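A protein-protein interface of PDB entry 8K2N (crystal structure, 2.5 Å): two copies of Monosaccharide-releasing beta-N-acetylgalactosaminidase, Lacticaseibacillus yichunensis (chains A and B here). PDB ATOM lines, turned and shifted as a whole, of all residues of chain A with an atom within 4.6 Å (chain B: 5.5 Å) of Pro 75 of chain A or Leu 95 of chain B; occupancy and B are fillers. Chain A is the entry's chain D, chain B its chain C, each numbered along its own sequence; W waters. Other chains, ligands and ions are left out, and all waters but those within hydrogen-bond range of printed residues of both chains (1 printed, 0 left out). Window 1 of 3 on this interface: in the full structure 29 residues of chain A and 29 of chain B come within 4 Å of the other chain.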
ATOM      1  N   GLN A  73      29.422 -18.022   3.448  1.00  0.00           N
ATOM      2  CA  GLN A  73      28.654 -17.623   2.290  1.00  0.00           C
ATOM      3  C   GLN A  73      27.155 -17.620   2.617  1.00  0.00           C
ATOM      4  O   GLN A  73      26.603 -18.593   3.184  1.00  0.00           O
ATOM      5  CB  GLN A  73      28.949 -18.535   1.102  1.00  0.00           C
ATOM      6  CG  GLN A  73      29.758 -17.885  -0.027  1.00  0.00           C
ATOM      7  CD  GLN A  73      31.193 -17.774   0.271  1.00  0.00           C
ATOM      8  OE1 GLN A  73      31.659 -18.144   1.316  1.00  0.00           O
ATOM      9  NE2 GLN A  73      31.936 -17.268  -0.665  1.00  0.00           N
ATOM     10  N   VAL A  74      26.517 -16.480   2.216  1.00  0.00           N
ATOM     11  CA  VAL A  74      25.099 -16.223   2.406  1.00  0.00           C
ATOM     12  C   VAL A  74      24.399 -15.890   1.068  1.00  0.00           C
ATOM     13  O   VAL A  74      24.904 -15.187   0.168  1.00  0.00           O
ATOM     14  CB  VAL A  74      24.836 -15.138   3.479  1.00  0.00           C
ATOM     15  CG1 VAL A  74      25.353 -15.527   4.855  1.00  0.00           C
ATOM     16  CG2 VAL A  74      25.433 -13.822   3.119  1.00  0.00           C
ATOM     17  N   PRO A  75      23.125 -16.328   0.913  1.00  0.00           N
ATOM     18  CA  PRO A  75      22.409 -16.037  -0.327  1.00  0.00           C
ATOM     19  C   PRO A  75      22.041 -14.565  -0.608  1.00  0.00           C
ATOM     20  O   PRO A  75      21.698 -13.813   0.318  1.00  0.00           O
ATOM     21  CB  PRO A  75      21.110 -16.855  -0.159  1.00  0.00           C
ATOM     22  CG  PRO A  75      20.995 -17.280   1.327  1.00  0.00           C
ATOM     23  CD  PRO A  75      22.308 -16.988   1.958  1.00  0.00           C
ATOM     24  N   SER A  76      22.025 -14.179  -1.904  1.00  0.00           N
ATOM     25  CA  SER A  76      21.383 -12.943  -2.385  1.00  0.00           C
ATOM     26  C   SER A  76      20.486 -13.153  -3.621  1.00  0.00           C
ATOM     27  O   SER A  76      20.965 -13.583  -4.660  1.00  0.00           O
ATOM     28  CB  SER A  76      22.408 -11.944  -2.711  1.00  0.00           C
ATOM     29  OG  SER A  76      21.727 -10.805  -3.177  1.00  0.00           O
ATOM     30  N   GLN A  77      19.205 -12.792  -3.563  1.00  0.00           N
ATOM     31  CA  GLN A  77      18.307 -12.786  -4.714  1.00  0.00           C
ATOM     32  C   GLN A  77      18.188 -11.402  -5.387  1.00  0.00           C
ATOM     33  O   GLN A  77      17.510 -11.214  -6.377  1.00  0.00           O
ATOM     34  CB  GLN A  77      16.948 -13.278  -4.206  1.00  0.00           C
ATOM     35  CG  GLN A  77      16.978 -14.755  -3.794  1.00  0.00           C
ATOM     36  CD  GLN A  77      16.741 -15.710  -4.940  1.00  0.00           C
ATOM     37  OE1 GLN A  77      15.622 -16.021  -5.390  1.00  0.00           O
ATOM     38  NE2 GLN A  77      17.865 -16.216  -5.418  1.00  0.00           N
ATOM     39  N   PRO A  93      21.880 -13.306  -8.968  1.00  0.00           N
ATOM     40  CA  PRO A  93      21.690 -14.099  -7.756  1.00  0.00           C
ATOM     41  C   PRO A  93      22.716 -15.208  -7.582  1.00  0.00           C
ATOM     42  O   PRO A  93      22.975 -15.943  -8.497  1.00  0.00           O
ATOM     43  CB  PRO A  93      20.254 -14.665  -7.940  1.00  0.00           C
ATOM     44  CG  PRO A  93      19.549 -13.556  -8.713  1.00  0.00           C
ATOM     45  CD  PRO A  93      20.605 -13.154  -9.710  1.00  0.00           C
ATOM     46  N   GLY A  94      23.301 -15.257  -6.388  1.00  0.00           N
ATOM     47  CA  GLY A  94      24.340 -16.197  -6.027  1.00  0.00           C
ATOM     48  C   GLY A  94      24.577 -16.112  -4.516  1.00  0.00           C
ATOM     49  O   GLY A  94      23.718 -15.621  -3.785  1.00  0.00           O
ATOM     50  N   LEU A  95      25.726 -16.659  -4.090  1.00  0.00           N
ATOM     51  CA  LEU A  95      26.237 -16.611  -2.731  1.00  0.00           C
ATOM     52  C   LEU A  95      27.326 -15.545  -2.635  1.00  0.00           C
ATOM     53  O   LEU A  95      28.164 -15.426  -3.514  1.00  0.00           O
ATOM     54  CB  LEU A  95      26.861 -17.963  -2.330  1.00  0.00           C
ATOM     55  CG  LEU A  95      25.935 -19.187  -2.310  1.00  0.00           C
ATOM     56  CD1 LEU A  95      26.717 -20.432  -1.922  1.00  0.00           C
ATOM     57  CD2 LEU A  95      24.831 -18.999  -1.322  1.00  0.00           C
ATOM     58  N   PHE A 409      26.471  -6.447  -0.597  1.00  0.00           N
ATOM     59  CA  PHE A 409      27.271  -7.672  -0.838  1.00  0.00           C
ATOM     60  C   PHE A 409      28.057  -7.666  -2.172  1.00  0.00           C
ATOM     61  O   PHE A 409      29.181  -8.210  -2.285  1.00  0.00           O
ATOM     62  CB  PHE A 409      26.408  -8.939  -0.887  1.00  0.00           C
ATOM     63  CG  PHE A 409      25.824  -9.419   0.413  1.00  0.00           C
ATOM     64  CD1 PHE A 409      26.048  -8.757   1.607  1.00  0.00           C
ATOM     65  CD2 PHE A 409      25.008 -10.565   0.434  1.00  0.00           C
ATOM     66  CE1 PHE A 409      25.440  -9.191   2.788  1.00  0.00           C
ATOM     67  CE2 PHE A 409      24.384 -10.995   1.603  1.00  0.00           C
ATOM     68  CZ  PHE A 409      24.585 -10.284   2.784  1.00  0.00           C
ATOM     69  N   PHE A 451      19.143 -15.314   7.722  1.00  0.00           N
ATOM     70  CA  PHE A 451      20.156 -16.240   7.196  1.00  0.00           C
ATOM     71  C   PHE A 451      19.824 -16.686   5.748  1.00  0.00           C
ATOM     72  O   PHE A 451      20.697 -17.005   4.956  1.00  0.00           O
ATOM     73  CB  PHE A 451      20.300 -17.414   8.176  1.00  0.00           C
ATOM     74  CG  PHE A 451      20.843 -17.079   9.550  1.00  0.00           C
ATOM     75  CD1 PHE A 451      22.206 -16.895   9.745  1.00  0.00           C
ATOM     76  CD2 PHE A 451      19.983 -16.928  10.648  1.00  0.00           C
ATOM     77  CE1 PHE A 451      22.700 -16.572  10.990  1.00  0.00           C
ATOM     78  CE2 PHE A 451      20.489 -16.665  11.910  1.00  0.00           C
ATOM     79  CZ  PHE A 451      21.829 -16.444  12.063  1.00  0.00           C
ATOM     80  N   ALA A 452      18.532 -16.701   5.366  1.00  0.00           N
ATOM     81  CA  ALA A 452      18.062 -17.095   4.022  1.00  0.00           C
ATOM     82  C   ALA A 452      17.729 -15.936   3.084  1.00  0.00           C
ATOM     83  O   ALA A 452      17.693 -16.171   1.897  1.00  0.00           O
ATOM     84  CB  ALA A 452      16.834 -17.921   4.196  1.00  0.00           C
ATOM     85  N   THR A 454      18.497 -11.749   2.511  1.00  0.00           N
ATOM     86  CA  THR A 454      19.338 -10.595   2.801  1.00  0.00           C
ATOM     87  C   THR A 454      18.941  -9.326   2.045  1.00  0.00           C
ATOM     88  O   THR A 454      19.619  -8.317   2.223  1.00  0.00           O
ATOM     89  CB  THR A 454      20.792 -10.970   2.482  1.00  0.00           C
ATOM     90  OG1 THR A 454      20.980 -11.020   1.060  1.00  0.00           O
ATOM     91  CG2 THR A 454      21.187 -12.282   3.145  1.00  0.00           C
ATOM     92  N   PHE B  18      17.765 -22.210 -13.483  1.00  0.00           N
ATOM     93  CA  PHE B  18      18.621 -21.371 -12.631  1.00  0.00           C
ATOM     94  C   PHE B  18      18.319 -19.887 -12.886  1.00  0.00           C
ATOM     95  O   PHE B  18      17.777 -19.539 -13.963  1.00  0.00           O
ATOM     96  CB  PHE B  18      20.092 -21.741 -12.821  1.00  0.00           C
ATOM     97  CG  PHE B  18      20.423 -23.115 -12.299  1.00  0.00           C
ATOM     98  CD1 PHE B  18      20.762 -23.296 -10.952  1.00  0.00           C
ATOM     99  CD2 PHE B  18      20.318 -24.238 -13.114  1.00  0.00           C
ATOM    100  CE1 PHE B  18      21.023 -24.565 -10.452  1.00  0.00           C
ATOM    101  CE2 PHE B  18      20.588 -25.507 -12.615  1.00  0.00           C
ATOM    102  CZ  PHE B  18      20.956 -25.663 -11.287  1.00  0.00           C
ATOM    103  N   GLN B  73      14.705 -20.238  -5.173  1.00  0.00           N
ATOM    104  CA  GLN B  73      16.108 -20.596  -5.214  1.00  0.00           C
ATOM    105  C   GLN B  73      16.620 -20.732  -3.789  1.00  0.00           C
ATOM    106  O   GLN B  73      16.478 -19.765  -3.054  1.00  0.00           O
ATOM    107  CB  GLN B  73      16.951 -19.545  -5.934  1.00  0.00           C
ATOM    108  CG  GLN B  73      16.655 -19.379  -7.438  1.00  0.00           C
ATOM    109  CD  GLN B  73      16.974 -20.499  -8.384  1.00  0.00           C
ATOM    110  OE1 GLN B  73      17.795 -21.376  -8.130  1.00  0.00           O
ATOM    111  NE2 GLN B  73      16.287 -20.468  -9.508  1.00  0.00           N
ATOM    112  N   VAL B  74      17.356 -21.840  -3.486  1.00  0.00           N
ATOM    113  CA  VAL B  74      17.812 -22.198  -2.138  1.00  0.00           C
ATOM    114  C   VAL B  74      19.338 -22.461  -2.117  1.00  0.00           C
ATOM    115  O   VAL B  74      19.921 -22.968  -3.068  1.00  0.00           O
ATOM    116  CB  VAL B  74      16.905 -23.342  -1.630  1.00  0.00           C
ATOM    117  CG1 VAL B  74      17.357 -23.996  -0.340  1.00  0.00           C
ATOM    118  CG2 VAL B  74      15.482 -22.841  -1.433  1.00  0.00           C
ATOM    119  N   PRO B  75      20.090 -22.026  -1.078  1.00  0.00           N
ATOM    120  CA  PRO B  75      21.530 -22.228  -1.069  1.00  0.00           C
ATOM    121  C   PRO B  75      22.024 -23.652  -0.819  1.00  0.00           C
ATOM    122  O   PRO B  75      21.466 -24.324   0.038  1.00  0.00           O
ATOM    123  CB  PRO B  75      21.951 -21.331   0.123  1.00  0.00           C
ATOM    124  CG  PRO B  75      20.840 -21.467   1.050  1.00  0.00           C
ATOM    125  CD  PRO B  75      19.665 -21.278   0.123  1.00  0.00           C
ATOM    126  N   SER B  76      23.139 -24.028  -1.490  1.00  0.00           N
ATOM    127  CA  SER B  76      23.910 -25.246  -1.216  1.00  0.00           C
ATOM    128  C   SER B  76      25.407 -24.915  -1.094  1.00  0.00           C
ATOM    129  O   SER B  76      25.997 -24.403  -2.064  1.00  0.00           O
ATOM    130  CB  SER B  76      23.715 -26.301  -2.321  1.00  0.00           C
ATOM    131  OG  SER B  76      24.612 -27.388  -2.176  1.00  0.00           O
ATOM    132  N   ARG B  90      25.570 -28.682 -11.952  1.00  0.00           N
ATOM    133  CA  ARG B  90      26.604 -27.821 -11.399  1.00  0.00           C
ATOM    134  C   ARG B  90      27.197 -28.520 -10.181  1.00  0.00           C
ATOM    135  O   ARG B  90      26.514 -29.289  -9.497  1.00  0.00           O
ATOM    136  CB  ARG B  90      26.008 -26.470 -10.958  1.00  0.00           C
ATOM    137  CG  ARG B  90      25.230 -25.761 -12.058  1.00  0.00           C
ATOM    138  CD  ARG B  90      24.729 -24.383 -11.642  1.00  0.00           C
ATOM    139  NE  ARG B  90      24.078 -23.766 -12.770  1.00  0.00           N
ATOM    140  CZ  ARG B  90      23.613 -22.520 -12.798  1.00  0.00           C
ATOM    141  NH1 ARG B  90      23.693 -21.738 -11.754  1.00  0.00           N
ATOM    142  NH2 ARG B  90      23.020 -22.046 -13.869  1.00  0.00           N
ATOM    143  N   PRO B  93      29.346 -24.507  -4.791  1.00  0.00           N
ATOM    144  CA  PRO B  93      28.322 -23.725  -4.049  1.00  0.00           C
ATOM    145  C   PRO B  93      27.629 -22.640  -4.878  1.00  0.00           C
ATOM    146  O   PRO B  93      28.264 -21.940  -5.634  1.00  0.00           O
ATOM    147  CB  PRO B  93      29.063 -23.133  -2.842  1.00  0.00           C
ATOM    148  CG  PRO B  93      30.307 -24.066  -2.655  1.00  0.00           C
ATOM    149  CD  PRO B  93      30.642 -24.618  -4.043  1.00  0.00           C
ATOM    150  N   GLY B  94      26.298 -22.599  -4.830  1.00  0.00           N
ATOM    151  CA  GLY B  94      25.481 -21.602  -5.495  1.00  0.00           C
ATOM    152  C   GLY B  94      24.034 -21.741  -5.011  1.00  0.00           C
ATOM    153  O   GLY B  94      23.756 -22.349  -3.978  1.00  0.00           O
ATOM    154  N   LEU B  95      23.086 -21.252  -5.803  1.00  0.00           N
ATOM    155  CA  LEU B  95      21.665 -21.349  -5.499  1.00  0.00           C
ATOM    156  C   LEU B  95      21.029 -22.430  -6.372  1.00  0.00           C
ATOM    157  O   LEU B  95      21.336 -22.552  -7.570  1.00  0.00           O
ATOM    158  CB  LEU B  95      21.006 -19.984  -5.773  1.00  0.00           C
ATOM    159  CG  LEU B  95      21.487 -18.780  -4.945  1.00  0.00           C
ATOM    160  CD1 LEU B  95      20.626 -17.519  -5.175  1.00  0.00           C
ATOM    161  CD2 LEU B  95      21.440 -19.069  -3.457  1.00  0.00           C
ATOM    162  N   PHE B  96      20.067 -23.185  -5.804  1.00  0.00           N
ATOM    163  CA  PHE B  96      19.434 -24.224  -6.604  1.00  0.00           C
ATOM    164  C   PHE B  96      17.921 -24.060  -6.456  1.00  0.00           C
ATOM    165  O   PHE B  96      17.452 -23.688  -5.347  1.00  0.00           O
ATOM    166  CB  PHE B  96      19.965 -25.605  -6.175  1.00  0.00           C
ATOM    167  CG  PHE B  96      21.424 -25.841  -6.479  1.00  0.00           C
ATOM    168  CD1 PHE B  96      22.423 -25.198  -5.752  1.00  0.00           C
ATOM    169  CD2 PHE B  96      21.818 -26.648  -7.548  1.00  0.00           C
ATOM    170  CE1 PHE B  96      23.777 -25.346  -6.089  1.00  0.00           C
ATOM    171  CE2 PHE B  96      23.177 -26.798  -7.875  1.00  0.00           C
ATOM    172  CZ  PHE B  96      24.148 -26.144  -7.154  1.00  0.00           C
ATOM    173  N   PRO B  97      17.135 -24.282  -7.559  1.00  0.00           N
ATOM    174  CA  PRO B  97      15.682 -24.192  -7.518  1.00  0.00           C
ATOM    175  C   PRO B  97      15.166 -25.416  -6.776  1.00  0.00           C
ATOM    176  O   PRO B  97      15.533 -26.543  -7.212  1.00  0.00           O
ATOM    177  CB  PRO B  97      15.234 -24.130  -8.992  1.00  0.00           C
ATOM    178  CG  PRO B  97      16.316 -24.910  -9.708  1.00  0.00           C
ATOM    179  CD  PRO B  97      17.570 -24.567  -8.936  1.00  0.00           C
HETATM  180  O   HOH W   1      13.497 -17.356  -6.103  1.00  0.00           O
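O of Pro 75 of chain A lies within hydrogen-bond range of OG1 of Thr 454 of chain A, at 3.0 Å.
The backbone carbonyl oxygen of Gly 94 of chain A lies within hydrogen-bond range of the backbone NH of Ser 76 of chain A (2.9 Å).
The backbone NH (N) of Ser 76 of chain B sits at hydrogen-bond distance from the backbone carbonyl oxygen (O) of Gly 94 of chain B (3.1 Å).
Leu 95 of chain B touches Pro 75 of chain A (CD2 to CB, 3.99 Å).
Leu 95 of chain B touches Ser 76 of chain A.
Gln 77 of chain A touches Gln 73 of chain B.
Leu 95 of chain B touches Gln 77 of chain A.
C of Pro 93 of chain A touches CD1 of Leu 95 of chain B, at 3.9 Å.
Gly 94 of chain A touches Leu 95 of chain B.
Pro 75 of chain B touches Leu 95 of chain A.
Pro 93 of chain B touches Leu 95 of chain A (CB to CD1, 3.7 Å).
Leu 95 of chain A touches Gly 94 of chain B (CD1 to N, 3.7 Å).
Of the printed residues of chain B, Pro 75 of chain A touches Leu 95.
Of the printed residues of chain B, Gln 77 of chain A touches Gln 73 (3.5 Å) and Leu 95 (3.1 Å).
Of the printed residues of chain A, Gln 73 of chain B touches Gln 77.
Of the printed residues of chain A, Pro 75 of chain B touches Leu 95.
Printed residues of chain A within 4 Å of Pro 93 of chain B: Leu 95 (3.7 Å).
Of the printed residues of chain A, Gly 94 of chain B touches Leu 95.
Of the printed residues of chain A, Leu 95 of chain B touches Pro 75, Ser 76, Gln 77, Pro 93 and Gly 94.
The nearest printed residue of chain B that does not touch Gly 94 of chain A is Gly 94 of chain B (5.5 Å).
Hydrophobic or aromatic side chains of chain B that line the printed part of chain A: Pro 75, Pro 93 and Leu 95.
Among the printed residues, 9 pairs touch across the chains.
Pro 75 of chain A touches Leu 95 of chain B, and with the chains exchanged Leu 95 of chain A touches Pro 75 of chain B.
Ser 76 of chain A touches Leu 95 of chain B, but with the chains exchanged Leu 95 of chain A does not touch Ser 76 of chain B (4.04 Å).
Pro 93 of chain A touches Leu 95 of chain B, and with the chains exchanged Leu 95 of chain A touches Pro 93 of chain B.
Gly 94 of chain A touches Leu 95 of chain B, and with the chains exchanged Leu 95 of chain A touches Gly 94 of chain B.
7 positions are printed for both chains.
Of the 9 pairs that touch across the chains among the printed residues, 6 have their exchanged pair printed and touching as well.
Water W1 bridges OE1 of Gln 77 of chain A (2.6 Å) and N of Gln 73 of chain B (3.3 Å).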
